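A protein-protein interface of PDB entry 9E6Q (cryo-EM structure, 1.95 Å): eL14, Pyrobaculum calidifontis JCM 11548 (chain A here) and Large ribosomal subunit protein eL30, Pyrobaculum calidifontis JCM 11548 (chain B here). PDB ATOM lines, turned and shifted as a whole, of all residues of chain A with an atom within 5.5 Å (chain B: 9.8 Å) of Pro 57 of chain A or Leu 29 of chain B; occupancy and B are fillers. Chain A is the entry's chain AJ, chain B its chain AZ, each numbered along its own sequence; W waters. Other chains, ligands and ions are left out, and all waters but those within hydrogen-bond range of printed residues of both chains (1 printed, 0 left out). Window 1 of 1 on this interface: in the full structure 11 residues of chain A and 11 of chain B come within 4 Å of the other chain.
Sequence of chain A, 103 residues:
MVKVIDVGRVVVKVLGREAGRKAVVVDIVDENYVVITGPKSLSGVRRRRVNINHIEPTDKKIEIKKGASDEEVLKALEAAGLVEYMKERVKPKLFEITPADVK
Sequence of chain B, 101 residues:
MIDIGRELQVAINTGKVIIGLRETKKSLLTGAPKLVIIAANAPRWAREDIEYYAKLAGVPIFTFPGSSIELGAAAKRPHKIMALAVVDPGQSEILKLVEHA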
ATOM      1  N   LYS A   3     -20.385 -12.439  -9.147  1.00  0.00           N
ATOM      2  CA  LYS A   3     -20.867 -13.615  -9.860  1.00  0.00           C
ATOM      3  C   LYS A   3     -22.301 -13.408 -10.337  1.00  0.00           C
ATOM      4  O   LYS A   3     -23.098 -12.749  -9.675  1.00  0.00           O
ATOM      5  CB  LYS A   3     -20.763 -14.860  -8.977  1.00  0.00           C
ATOM      6  CG  LYS A   3     -21.933 -15.066  -8.037  1.00  0.00           C
ATOM      7  CD  LYS A   3     -21.517 -15.805  -6.782  1.00  0.00           C
ATOM      8  CE  LYS A   3     -20.612 -16.980  -7.091  1.00  0.00           C
ATOM      9  NZ  LYS A   3     -21.387 -18.114  -7.646  1.00  0.00           N
ATOM     10  N   VAL A   4     -22.613 -13.955 -11.508  1.00  0.00           N
ATOM     11  CA  VAL A   4     -23.960 -13.834 -12.049  1.00  0.00           C
ATOM     12  C   VAL A   4     -24.784 -15.064 -11.710  1.00  0.00           C
ATOM     13  O   VAL A   4     -25.913 -14.960 -11.219  1.00  0.00           O
ATOM     14  CB  VAL A   4     -23.907 -13.602 -13.569  1.00  0.00           C
ATOM     15  CG1 VAL A   4     -25.295 -13.686 -14.153  1.00  0.00           C
ATOM     16  CG2 VAL A   4     -23.281 -12.267 -13.879  1.00  0.00           C
ATOM     17  N   ILE A   5     -24.232 -16.247 -11.959  1.00  0.00           N
ATOM     18  CA  ILE A   5     -24.955 -17.499 -11.753  1.00  0.00           C
ATOM     19  C   ILE A   5     -24.828 -17.810 -10.266  1.00  0.00           C
ATOM     20  O   ILE A   5     -23.883 -18.452  -9.816  1.00  0.00           O
ATOM     21  CB  ILE A   5     -24.416 -18.620 -12.634  1.00  0.00           C
ATOM     22  CG1 ILE A   5     -24.637 -18.280 -14.105  1.00  0.00           C
ATOM     23  CG2 ILE A   5     -25.127 -19.920 -12.323  1.00  0.00           C
ATOM     24  CD1 ILE A   5     -26.059 -17.942 -14.436  1.00  0.00           C
ATOM     25  N   ARG A   9     -30.716 -16.637  -8.967  1.00  0.00           N
ATOM     26  CA  ARG A   9     -30.679 -16.081 -10.311  1.00  0.00           C
ATOM     27  C   ARG A   9     -31.539 -16.928 -11.238  1.00  0.00           C
ATOM     28  O   ARG A   9     -31.345 -18.143 -11.336  1.00  0.00           O
ATOM     29  CB  ARG A   9     -29.243 -16.013 -10.818  1.00  0.00           C
ATOM     30  CG  ARG A   9     -29.126 -15.888 -12.316  1.00  0.00           C
ATOM     31  CD  ARG A   9     -29.377 -14.468 -12.751  1.00  0.00           C
ATOM     32  NE  ARG A   9     -28.382 -13.556 -12.205  1.00  0.00           N
ATOM     33  CZ  ARG A   9     -28.538 -12.244 -12.121  1.00  0.00           C
ATOM     34  NH1 ARG A   9     -29.639 -11.651 -12.551  1.00  0.00           N
ATOM     35  NH2 ARG A   9     -27.564 -11.509 -11.597  1.00  0.00           N
ATOM     36  N   VAL A  10     -32.502 -16.291 -11.902  1.00  0.00           N
ATOM     37  CA  VAL A  10     -33.365 -16.995 -12.840  1.00  0.00           C
ATOM     38  C   VAL A  10     -32.625 -17.221 -14.151  1.00  0.00           C
ATOM     39  O   VAL A  10     -32.002 -16.305 -14.702  1.00  0.00           O
ATOM     40  CB  VAL A  10     -34.667 -16.210 -13.062  1.00  0.00           C
ATOM     41  CG1 VAL A  10     -35.476 -16.829 -14.175  1.00  0.00           C
ATOM     42  CG2 VAL A  10     -35.476 -16.168 -11.787  1.00  0.00           C
ATOM     43  N   VAL A  11     -32.692 -18.448 -14.662  1.00  0.00           N
ATOM     44  CA  VAL A  11     -31.972 -18.833 -15.865  1.00  0.00           C
ATOM     45  C   VAL A  11     -32.928 -19.500 -16.842  1.00  0.00           C
ATOM     46  O   VAL A  11     -34.016 -19.947 -16.480  1.00  0.00           O
ATOM     47  CB  VAL A  11     -30.794 -19.774 -15.555  1.00  0.00           C
ATOM     48  CG1 VAL A  11     -29.801 -19.093 -14.648  1.00  0.00           C
ATOM     49  CG2 VAL A  11     -31.299 -21.057 -14.931  1.00  0.00           C
ATOM     50  N   VAL A  12     -32.503 -19.553 -18.098  1.00  0.00           N
ATOM     51  CA  VAL A  12     -33.211 -20.259 -19.157  1.00  0.00           C
ATOM     52  C   VAL A  12     -32.269 -21.313 -19.712  1.00  0.00           C
ATOM     53  O   VAL A  12     -31.191 -20.979 -20.217  1.00  0.00           O
ATOM     54  CB  VAL A  12     -33.670 -19.305 -20.269  1.00  0.00           C
ATOM     55  CG1 VAL A  12     -34.294 -20.082 -21.404  1.00  0.00           C
ATOM     56  CG2 VAL A  12     -34.640 -18.283 -19.724  1.00  0.00           C
ATOM     57  N   ILE A  52     -22.970 -24.898 -16.315  1.00  0.00           N
ATOM     58  CA  ILE A  52     -23.223 -23.466 -16.421  1.00  0.00           C
ATOM     59  C   ILE A  52     -23.207 -23.001 -17.865  1.00  0.00           C
ATOM     60  O   ILE A  52     -23.758 -21.945 -18.179  1.00  0.00           O
ATOM     61  CB  ILE A  52     -22.211 -22.662 -15.586  1.00  0.00           C
ATOM     62  CG1 ILE A  52     -20.788 -22.994 -16.014  1.00  0.00           C
ATOM     63  CG2 ILE A  52     -22.399 -22.947 -14.117  1.00  0.00           C
ATOM     64  CD1 ILE A  52     -19.942 -21.786 -16.284  1.00  0.00           C
ATOM     65  N   ILE A  55     -26.978 -22.985 -19.500  1.00  0.00           N
ATOM     66  CA  ILE A  55     -28.019 -22.078 -19.040  1.00  0.00           C
ATOM     67  C   ILE A  55     -27.611 -20.660 -19.396  1.00  0.00           C
ATOM     68  O   ILE A  55     -26.431 -20.305 -19.315  1.00  0.00           O
ATOM     69  CB  ILE A  55     -28.275 -22.196 -17.524  1.00  0.00           C
ATOM     70  CG1 ILE A  55     -26.954 -22.204 -16.759  1.00  0.00           C
ATOM     71  CG2 ILE A  55     -29.116 -23.425 -17.219  1.00  0.00           C
ATOM     72  CD1 ILE A  55     -27.112 -22.080 -15.279  1.00  0.00           C
ATOM     73  N   GLU A  56     -28.582 -19.859 -19.819  1.00  0.00           N
ATOM     74  CA  GLU A  56     -28.351 -18.448 -20.061  1.00  0.00           C
ATOM     75  C   GLU A  56     -28.963 -17.648 -18.928  1.00  0.00           C
ATOM     76  O   GLU A  56     -30.161 -17.811 -18.651  1.00  0.00           O
ATOM     77  CB  GLU A  56     -28.946 -18.022 -21.395  1.00  0.00           C
ATOM     78  CG  GLU A  56     -28.941 -16.526 -21.633  1.00  0.00           C
ATOM     79  CD  GLU A  56     -27.659 -16.023 -22.268  1.00  0.00           C
ATOM     80  OE1 GLU A  56     -26.649 -16.755 -22.252  1.00  0.00           O
ATOM     81  OE2 GLU A  56     -27.657 -14.889 -22.786  1.00  0.00           O
ATOM     82  N   PRO A  57     -28.200 -16.815 -18.231  1.00  0.00           N
ATOM     83  CA  PRO A  57     -28.776 -16.043 -17.128  1.00  0.00           C
ATOM     84  C   PRO A  57     -29.761 -15.000 -17.617  1.00  0.00           C
ATOM     85  O   PRO A  57     -29.664 -14.482 -18.730  1.00  0.00           O
ATOM     86  CB  PRO A  57     -27.559 -15.385 -16.474  1.00  0.00           C
ATOM     87  CG  PRO A  57     -26.515 -15.385 -17.498  1.00  0.00           C
ATOM     88  CD  PRO A  57     -26.790 -16.479 -18.476  1.00  0.00           C
ATOM     89  N   THR A  58     -30.719 -14.695 -16.757  1.00  0.00           N
ATOM     90  CA  THR A  58     -31.690 -13.638 -16.978  1.00  0.00           C
ATOM     91  C   THR A  58     -31.393 -12.497 -16.010  1.00  0.00           C
ATOM     92  O   THR A  58     -30.786 -12.691 -14.957  1.00  0.00           O
ATOM     93  CB  THR A  58     -33.111 -14.183 -16.789  1.00  0.00           C
ATOM     94  OG1 THR A  58     -33.391 -15.144 -17.811  1.00  0.00           O
ATOM     95  CG2 THR A  58     -34.145 -13.089 -16.885  1.00  0.00           C
ATOM     96  N   ASP A  59     -31.798 -11.286 -16.389  1.00  0.00           N
ATOM     97  CA  ASP A  59     -31.629 -10.143 -15.505  1.00  0.00           C
ATOM     98  C   ASP A  59     -32.496 -10.209 -14.249  1.00  0.00           C
ATOM     99  O   ASP A  59     -32.295  -9.399 -13.342  1.00  0.00           O
ATOM    100  CB  ASP A  59     -31.879  -8.840 -16.279  1.00  0.00           C
ATOM    101  CG  ASP A  59     -33.338  -8.628 -16.655  1.00  0.00           C
ATOM    102  OD1 ASP A  59     -33.609  -7.667 -17.402  1.00  0.00           O
ATOM    103  OD2 ASP A  59     -34.211  -9.418 -16.251  1.00  0.00           O
ATOM    104  N   ILE B  18      -6.853 -14.051 -16.877  1.00  0.00           N
ATOM    105  CA  ILE B  18      -7.545 -15.166 -17.507  1.00  0.00           C
ATOM    106  C   ILE B  18      -7.633 -14.884 -18.997  1.00  0.00           C
ATOM    107  O   ILE B  18      -8.165 -13.849 -19.406  1.00  0.00           O
ATOM    108  CB  ILE B  18      -8.939 -15.358 -16.890  1.00  0.00           C
ATOM    109  CG1 ILE B  18      -8.805 -15.886 -15.464  1.00  0.00           C
ATOM    110  CG2 ILE B  18      -9.780 -16.276 -17.728  1.00  0.00           C
ATOM    111  CD1 ILE B  18     -10.117 -16.049 -14.756  1.00  0.00           C
ATOM    112  N   LEU B  21     -11.736 -16.497 -24.632  1.00  0.00           N
ATOM    113  CA  LEU B  21     -13.155 -16.170 -24.537  1.00  0.00           C
ATOM    114  C   LEU B  21     -13.893 -17.123 -23.606  1.00  0.00           C
ATOM    115  O   LEU B  21     -14.714 -16.690 -22.792  1.00  0.00           O
ATOM    116  CB  LEU B  21     -13.791 -16.194 -25.924  1.00  0.00           C
ATOM    117  CG  LEU B  21     -15.292 -15.905 -25.968  1.00  0.00           C
ATOM    118  CD1 LEU B  21     -15.596 -14.578 -25.310  1.00  0.00           C
ATOM    119  CD2 LEU B  21     -15.810 -15.931 -27.388  1.00  0.00           C
ATOM    120  N   ARG B  22     -13.628 -18.425 -23.718  1.00  0.00           N
ATOM    121  CA  ARG B  22     -14.377 -19.389 -22.920  1.00  0.00           C
ATOM    122  C   ARG B  22     -14.087 -19.227 -21.435  1.00  0.00           C
ATOM    123  O   ARG B  22     -15.002 -19.296 -20.610  1.00  0.00           O
ATOM    124  CB  ARG B  22     -14.070 -20.811 -23.380  1.00  0.00           C
ATOM    125  CG  ARG B  22     -14.995 -21.294 -24.472  1.00  0.00           C
ATOM    126  CD  ARG B  22     -14.534 -22.589 -25.092  1.00  0.00           C
ATOM    127  NE  ARG B  22     -14.367 -23.649 -24.108  1.00  0.00           N
ATOM    128  CZ  ARG B  22     -14.880 -24.866 -24.225  1.00  0.00           C
ATOM    129  NH1 ARG B  22     -15.615 -25.205 -25.269  1.00  0.00           N
ATOM    130  NH2 ARG B  22     -14.647 -25.764 -23.276  1.00  0.00           N
ATOM    131  N   GLU B  23     -12.824 -19.016 -21.070  1.00  0.00           N
ATOM    132  CA  GLU B  23     -12.493 -18.833 -19.664  1.00  0.00           C
ATOM    133  C   GLU B  23     -12.936 -17.469 -19.152  1.00  0.00           C
ATOM    134  O   GLU B  23     -13.292 -17.338 -17.978  1.00  0.00           O
ATOM    135  CB  GLU B  23     -10.997 -19.027 -19.447  1.00  0.00           C
ATOM    136  CG  GLU B  23     -10.518 -20.430 -19.725  1.00  0.00           C
ATOM    137  CD  GLU B  23     -10.335 -21.238 -18.468  1.00  0.00           C
ATOM    138  OE1 GLU B  23     -11.338 -21.783 -17.961  1.00  0.00           O
ATOM    139  OE2 GLU B  23      -9.190 -21.335 -17.985  1.00  0.00           O
ATOM    140  N   THR B  24     -12.914 -16.448 -20.007  1.00  0.00           N
ATOM    141  CA  THR B  24     -13.394 -15.132 -19.603  1.00  0.00           C
ATOM    142  C   THR B  24     -14.877 -15.172 -19.276  1.00  0.00           C
ATOM    143  O   THR B  24     -15.324 -14.581 -18.288  1.00  0.00           O
ATOM    144  CB  THR B  24     -13.116 -14.112 -20.704  1.00  0.00           C
ATOM    145  OG1 THR B  24     -11.707 -14.023 -20.930  1.00  0.00           O
ATOM    146  CG2 THR B  24     -13.646 -12.754 -20.317  1.00  0.00           C
ATOM    147  N   LYS B  25     -15.657 -15.874 -20.098  1.00  0.00           N
ATOM    148  CA  LYS B  25     -17.083 -16.023 -19.839  1.00  0.00           C
ATOM    149  C   LYS B  25     -17.328 -16.712 -18.508  1.00  0.00           C
ATOM    150  O   LYS B  25     -18.214 -16.314 -17.746  1.00  0.00           O
ATOM    151  CB  LYS B  25     -17.732 -16.820 -20.966  1.00  0.00           C
ATOM    152  CG  LYS B  25     -18.121 -16.011 -22.177  1.00  0.00           C
ATOM    153  CD  LYS B  25     -18.569 -16.930 -23.295  1.00  0.00           C
ATOM    154  CE  LYS B  25     -19.832 -16.430 -23.959  1.00  0.00           C
ATOM    155  NZ  LYS B  25     -20.310 -17.361 -25.017  1.00  0.00           N
ATOM    156  N   LYS B  26     -16.553 -17.754 -18.212  1.00  0.00           N
ATOM    157  CA  LYS B  26     -16.717 -18.463 -16.950  1.00  0.00           C
ATOM    158  C   LYS B  26     -16.380 -17.572 -15.765  1.00  0.00           C
ATOM    159  O   LYS B  26     -17.046 -17.632 -14.728  1.00  0.00           O
ATOM    160  CB  LYS B  26     -15.848 -19.715 -16.937  1.00  0.00           C
ATOM    161  CG  LYS B  26     -16.421 -20.853 -16.129  1.00  0.00           C
ATOM    162  CD  LYS B  26     -15.481 -22.043 -16.109  1.00  0.00           C
ATOM    163  CE  LYS B  26     -14.094 -21.663 -15.608  1.00  0.00           C
ATOM    164  NZ  LYS B  26     -14.134 -20.763 -14.424  1.00  0.00           N
ATOM    165  N   SER B  27     -15.336 -16.755 -15.889  1.00  0.00           N
ATOM    166  CA  SER B  27     -14.985 -15.846 -14.805  1.00  0.00           C
ATOM    167  C   SER B  27     -16.093 -14.828 -14.567  1.00  0.00           C
ATOM    168  O   SER B  27     -16.444 -14.535 -13.422  1.00  0.00           O
ATOM    169  CB  SER B  27     -13.666 -15.146 -15.115  1.00  0.00           C
ATOM    170  OG  SER B  27     -13.907 -13.849 -15.616  1.00  0.00           O
ATOM    171  N   LEU B  28     -16.657 -14.279 -15.641  1.00  0.00           N
ATOM    172  CA  LEU B  28     -17.759 -13.337 -15.490  1.00  0.00           C
ATOM    173  C   LEU B  28     -18.958 -13.999 -14.824  1.00  0.00           C
ATOM    174  O   LEU B  28     -19.579 -13.422 -13.927  1.00  0.00           O
ATOM    175  CB  LEU B  28     -18.149 -12.761 -16.850  1.00  0.00           C
ATOM    176  CG  LEU B  28     -17.264 -11.633 -17.376  1.00  0.00           C
ATOM    177  CD1 LEU B  28     -17.499 -11.414 -18.851  1.00  0.00           C
ATOM    178  CD2 LEU B  28     -17.528 -10.360 -16.601  1.00  0.00           C
ATOM    179  N   LEU B  29     -19.291 -15.220 -15.241  1.00  0.00           N
ATOM    180  CA  LEU B  29     -20.478 -15.887 -14.717  1.00  0.00           C
ATOM    181  C   LEU B  29     -20.263 -16.451 -13.320  1.00  0.00           C
ATOM    182  O   LEU B  29     -21.193 -16.448 -12.512  1.00  0.00           O
ATOM    183  CB  LEU B  29     -20.919 -17.009 -15.656  1.00  0.00           C
ATOM    184  CG  LEU B  29     -21.488 -16.600 -17.013  1.00  0.00           C
ATOM    185  CD1 LEU B  29     -21.534 -17.796 -17.944  1.00  0.00           C
ATOM    186  CD2 LEU B  29     -22.858 -15.984 -16.867  1.00  0.00           C
ATOM    187  N   THR B  30     -19.066 -16.939 -13.015  1.00  0.00           N
ATOM    188  CA  THR B  30     -18.819 -17.608 -11.747  1.00  0.00           C
ATOM    189  C   THR B  30     -17.884 -16.859 -10.813  1.00  0.00           C
ATOM    190  O   THR B  30     -18.102 -16.890  -9.603  1.00  0.00           O
ATOM    191  CB  THR B  30     -18.245 -19.011 -11.980  1.00  0.00           C
ATOM    192  OG1 THR B  30     -17.039 -18.916 -12.747  1.00  0.00           O
ATOM    193  CG2 THR B  30     -19.242 -19.866 -12.726  1.00  0.00           C
ATOM    194  N   GLY B  31     -16.848 -16.201 -11.329  1.00  0.00           N
ATOM    195  CA  GLY B  31     -15.918 -15.459 -10.509  1.00  0.00           C
ATOM    196  C   GLY B  31     -16.298 -13.996 -10.389  1.00  0.00           C
ATOM    197  O   GLY B  31     -17.412 -13.576 -10.706  1.00  0.00           O
ATOM    198  N   ALA B  32     -15.338 -13.205  -9.923  1.00  0.00           N
ATOM    199  CA  ALA B  32     -15.504 -11.762  -9.774  1.00  0.00           C
ATOM    200  C   ALA B  32     -14.316 -11.049 -10.408  1.00  0.00           C
ATOM    201  O   ALA B  32     -13.436 -10.536  -9.710  1.00  0.00           O
ATOM    202  CB  ALA B  32     -15.659 -11.377  -8.303  1.00  0.00           C
ATOM    203  N   PRO B  33     -14.260 -11.005 -11.736  1.00  0.00           N
ATOM    204  CA  PRO B  33     -13.201 -10.247 -12.400  1.00  0.00           C
ATOM    205  C   PRO B  33     -13.381  -8.753 -12.196  1.00  0.00           C
ATOM    206  O   PRO B  33     -14.485  -8.264 -11.949  1.00  0.00           O
ATOM    207  CB  PRO B  33     -13.377 -10.635 -13.870  1.00  0.00           C
ATOM    208  CG  PRO B  33     -14.844 -10.839 -13.973  1.00  0.00           C
ATOM    209  CD  PRO B  33     -15.171 -11.609 -12.723  1.00  0.00           C
ATOM    210  N   VAL B  36     -12.571  -6.655 -17.943  1.00  0.00           N
ATOM    211  CA  VAL B  36     -12.579  -7.524 -19.109  1.00  0.00           C
ATOM    212  C   VAL B  36     -12.140  -6.697 -20.306  1.00  0.00           C
ATOM    213  O   VAL B  36     -12.599  -5.567 -20.490  1.00  0.00           O
ATOM    214  CB  VAL B  36     -13.970  -8.147 -19.345  1.00  0.00           C
ATOM    215  CG1 VAL B  36     -14.079  -8.719 -20.742  1.00  0.00           C
ATOM    216  CG2 VAL B  36     -14.238  -9.219 -18.315  1.00  0.00           C
ATOM    217  N   ASP B  49     -22.244 -11.433 -26.194  1.00  0.00           N
ATOM    218  CA  ASP B  49     -22.202 -12.307 -25.027  1.00  0.00           C
ATOM    219  C   ASP B  49     -21.422 -11.666 -23.890  1.00  0.00           C
ATOM    220  O   ASP B  49     -21.884 -11.633 -22.746  1.00  0.00           O
ATOM    221  CB  ASP B  49     -21.582 -13.652 -25.404  1.00  0.00           C
ATOM    222  CG  ASP B  49     -22.595 -14.634 -25.951  1.00  0.00           C
ATOM    223  OD1 ASP B  49     -22.624 -15.783 -25.471  1.00  0.00           O
ATOM    224  OD2 ASP B  49     -23.362 -14.262 -26.857  1.00  0.00           O
ATOM    225  N   ILE B  50     -20.228 -11.149 -24.188  1.00  0.00           N
ATOM    226  CA  ILE B  50     -19.414 -10.511 -23.159  1.00  0.00           C
ATOM    227  C   ILE B  50     -20.090  -9.247 -22.649  1.00  0.00           C
ATOM    228  O   ILE B  50     -20.120  -8.988 -21.441  1.00  0.00           O
ATOM    229  CB  ILE B  50     -18.001 -10.225 -23.699  1.00  0.00           C
ATOM    230  CG1 ILE B  50     -17.247 -11.531 -23.919  1.00  0.00           C
ATOM    231  CG2 ILE B  50     -17.226  -9.351 -22.741  1.00  0.00           C
ATOM    232  CD1 ILE B  50     -16.999 -12.297 -22.651  1.00  0.00           C
ATOM    233  N   TYR B  52     -23.263  -8.577 -22.504  1.00  0.00           N
ATOM    234  CA  TYR B  52     -24.397  -8.945 -21.668  1.00  0.00           C
ATOM    235  C   TYR B  52     -23.941  -9.468 -20.313  1.00  0.00           C
ATOM    236  O   TYR B  52     -24.464  -9.059 -19.273  1.00  0.00           O
ATOM    237  CB  TYR B  52     -25.241  -9.992 -22.391  1.00  0.00           C
ATOM    238  CG  TYR B  52     -26.485 -10.408 -21.652  1.00  0.00           C
ATOM    239  CD1 TYR B  52     -27.456  -9.484 -21.309  1.00  0.00           C
ATOM    240  CD2 TYR B  52     -26.679 -11.729 -21.287  1.00  0.00           C
ATOM    241  CE1 TYR B  52     -28.587  -9.866 -20.633  1.00  0.00           C
ATOM    242  CE2 TYR B  52     -27.805 -12.117 -20.613  1.00  0.00           C
ATOM    243  CZ  TYR B  52     -28.756 -11.184 -20.287  1.00  0.00           C
ATOM    244  OH  TYR B  52     -29.885 -11.582 -19.611  1.00  0.00           O
ATOM    245  N   TYR B  53     -22.970 -10.381 -20.302  1.00  0.00           N
ATOM    246  CA  TYR B  53     -22.554 -10.995 -19.048  1.00  0.00           C
ATOM    247  C   TYR B  53     -21.830  -9.997 -18.159  1.00  0.00           C
ATOM    248  O   TYR B  53     -22.035  -9.984 -16.942  1.00  0.00           O
ATOM    249  CB  TYR B  53     -21.662 -12.202 -19.319  1.00  0.00           C
ATOM    250  CG  TYR B  53     -22.393 -13.361 -19.933  1.00  0.00           C
ATOM    251  CD1 TYR B  53     -23.760 -13.517 -19.754  1.00  0.00           C
ATOM    252  CD2 TYR B  53     -21.720 -14.302 -20.691  1.00  0.00           C
ATOM    253  CE1 TYR B  53     -24.433 -14.569 -20.318  1.00  0.00           C
ATOM    254  CE2 TYR B  53     -22.387 -15.364 -21.255  1.00  0.00           C
ATOM    255  CZ  TYR B  53     -23.744 -15.491 -21.066  1.00  0.00           C
ATOM    256  OH  TYR B  53     -24.420 -16.547 -21.626  1.00  0.00           O
ATOM    257  N   ALA B  54     -20.970  -9.164 -18.746  1.00  0.00           N
ATOM    258  CA  ALA B  54     -20.254  -8.168 -17.959  1.00  0.00           C
ATOM    259  C   ALA B  54     -21.209  -7.141 -17.374  1.00  0.00           C
ATOM    260  O   ALA B  54     -20.988  -6.638 -16.268  1.00  0.00           O
ATOM    261  CB  ALA B  54     -19.188  -7.483 -18.809  1.00  0.00           C
ATOM    262  N   LYS B  55     -22.270  -6.808 -18.106  1.00  0.00           N
ATOM    263  CA  LYS B  55     -23.279  -5.903 -17.570  1.00  0.00           C
ATOM    264  C   LYS B  55     -23.946  -6.503 -16.340  1.00  0.00           C
ATOM    265  O   LYS B  55     -23.984  -5.882 -15.274  1.00  0.00           O
ATOM    266  CB  LYS B  55     -24.316  -5.581 -18.641  1.00  0.00           C
ATOM    267  CG  LYS B  55     -25.614  -5.036 -18.082  1.00  0.00           C
ATOM    268  CD  LYS B  55     -26.804  -5.531 -18.873  1.00  0.00           C
ATOM    269  CE  LYS B  55     -26.983  -4.732 -20.145  1.00  0.00           C
ATOM    270  NZ  LYS B  55     -27.593  -3.405 -19.876  1.00  0.00           N
ATOM    271  N   LEU B  56     -24.458  -7.731 -16.463  1.00  0.00           N
ATOM    272  CA  LEU B  56     -25.095  -8.383 -15.325  1.00  0.00           C
ATOM    273  C   LEU B  56     -24.122  -8.616 -14.186  1.00  0.00           C
ATOM    274  O   LEU B  56     -24.549  -8.726 -13.033  1.00  0.00           O
ATOM    275  CB  LEU B  56     -25.716  -9.717 -15.742  1.00  0.00           C
ATOM    276  CG  LEU B  56     -26.756  -9.691 -16.856  1.00  0.00           C
ATOM    277  CD1 LEU B  56     -27.204 -11.095 -17.180  1.00  0.00           C
ATOM    278  CD2 LEU B  56     -27.931  -8.840 -16.446  1.00  0.00           C
ATOM    279  N   ALA B  57     -22.831  -8.701 -14.476  1.00  0.00           N
ATOM    280  CA  ALA B  57     -21.827  -8.868 -13.440  1.00  0.00           C
ATOM    281  C   ALA B  57     -21.303  -7.548 -12.899  1.00  0.00           C
ATOM    282  O   ALA B  57     -20.591  -7.554 -11.892  1.00  0.00           O
ATOM    283  CB  ALA B  57     -20.655  -9.695 -13.970  1.00  0.00           C
ATOM    284  N   GLY B  58     -21.640  -6.429 -13.531  1.00  0.00           N
ATOM    285  CA  GLY B  58     -21.108  -5.146 -13.122  1.00  0.00           C
ATOM    286  C   GLY B  58     -19.605  -5.055 -13.264  1.00  0.00           C
ATOM    287  O   GLY B  58     -18.912  -4.631 -12.337  1.00  0.00           O
ATOM    288  N   VAL B  59     -19.084  -5.476 -14.412  1.00  0.00           N
ATOM    289  CA  VAL B  59     -17.657  -5.447 -14.701  1.00  0.00           C
ATOM    290  C   VAL B  59     -17.453  -4.559 -15.920  1.00  0.00           C
ATOM    291  O   VAL B  59     -18.142  -4.740 -16.924  1.00  0.00           O
ATOM    292  CB  VAL B  59     -17.082  -6.852 -14.957  1.00  0.00           C
ATOM    293  CG1 VAL B  59     -15.569  -6.803 -15.054  1.00  0.00           C
ATOM    294  CG2 VAL B  59     -17.514  -7.798 -13.857  1.00  0.00           C
ATOM    295  N   ALA B  85      -9.726 -11.513 -19.054  1.00  0.00           N
ATOM    296  CA  ALA B  85     -10.304 -10.952 -17.841  1.00  0.00           C
ATOM    297  C   ALA B  85      -9.205 -10.726 -16.817  1.00  0.00           C
ATOM    298  O   ALA B  85      -8.454 -11.649 -16.495  1.00  0.00           O
ATOM    299  CB  ALA B  85     -11.381 -11.871 -17.263  1.00  0.00           C
HETATM  300  O   HOH W   1     -26.945  -8.561 -12.326  1.00  0.00           O
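The backbone carbonyl oxygen (O) of Ile 5 of chain A lies within hydrogen-bond range of the side-chain amino group (NZ) of Lys 3 of chain A, 3.3 Å away. O of Val 4 of chain A lies within hydrogen-bond range of NE of Arg 9 of chain A (3.0 Å). The backbone carbonyl oxygen of Thr 58 of chain A is in hydrogen-bond range of the guanidinium group of Arg 9 of chain A, 2.9 Å away. O of Val 10 of chain A lies within hydrogen-bond range of N of Thr 58 of chain A. N of Glu 56 of chain A lies within hydrogen-bond range of O of Val 12 of chain A, at 2.9 Å.
N of Val 4 of chain A lies within hydrogen-bond range of O of Leu 29 of chain B. N of Ile 5 of chain A is in hydrogen-bond range of O of Leu 29 of chain B, at 3.1 Å. O of Pro 57 of chain A is in hydrogen-bond range of OH of Tyr 52 of chain B, at 3.0 Å. OE1 of Glu 56 of chain A lies close to OH of Tyr 53 of chain B.
Of chain B, only Leu 29 (3.8 Å), Tyr 52 (3.0 Å) and Tyr 53 (3.5 Å) come within 4 Å of Pro 57 of chain A. Of chain A, only Lys 3, Val 4, Ile 5 and Pro 57 come within 4 Å of Leu 29 of chain B. Glu 56 of chain A touches just these residues of chain B: Tyr 52 (3.5 Å) and Tyr 53 (2.3 Å). Thr 58 of chain A touches just one residue of chain B: Tyr 52. Of the printed residues of chain A, Ala 57 of chain B touches Val 4. Printed residues of chain B within 4 Å of Val 4 of chain A: Leu 28, Leu 29, Leu 56 and Ala 57. Of the printed residues of chain A, Tyr 52 of chain B touches Glu 56, Pro 57, Thr 58 and Asp 59. Ile 55 of chain A touches none of the printed residues of chain B. Arg 22 of chain B touches none of the printed residues of chain A. The nearest residue of chain A that does not touch Leu 29 of chain B is Ile 52 of chain A (4.6 Å).
Water W1 lies within hydrogen-bond range of the backbone carbonyl oxygen of Leu 56 of chain B (2.5 Å) and the guanidinium group of Arg 9 of chain A (3.1 Å).
Among the printed residues, pairs that only touch across the chains: Lys 3 of chain A with Thr 30 of chain B, Glu 56 of chain A with Tyr 52 of chain B, Lys 3 of chain A with Gly 31 of chain B, Pro 57 of chain A with Tyr 53 of chain B, Val 4 of chain A with Ala 57 of chain B, Ile 52 of chain A with Lys 26 of chain B, Asp 59 of chain A with Tyr 52 of chain B, Pro 57 of chain A with Leu 29 of chain B, Val 4 of chain A with Leu 56 of chain B, Thr 58 of chain A with Tyr 52 of chain B, Val 4 of chain A with Leu 28 of chain B, Lys 3 of chain A with Leu 29 of chain B and Asp 59 of chain A with Leu 56 of chain B.
Of the 26 printed residues of chain B, 9 touch a printed residue of chain A. Printed residues of chain B that touch a printed residue of chain A: Lys 26, Leu 28, Leu 29, Thr 30, Gly 31, Tyr 52, Tyr 53, Leu 56 and Ala 57. Among the printed residues, no Asp or Glu carboxylate lies within 4 Å of a Lys or Arg side-chain nitrogen of the other chain.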
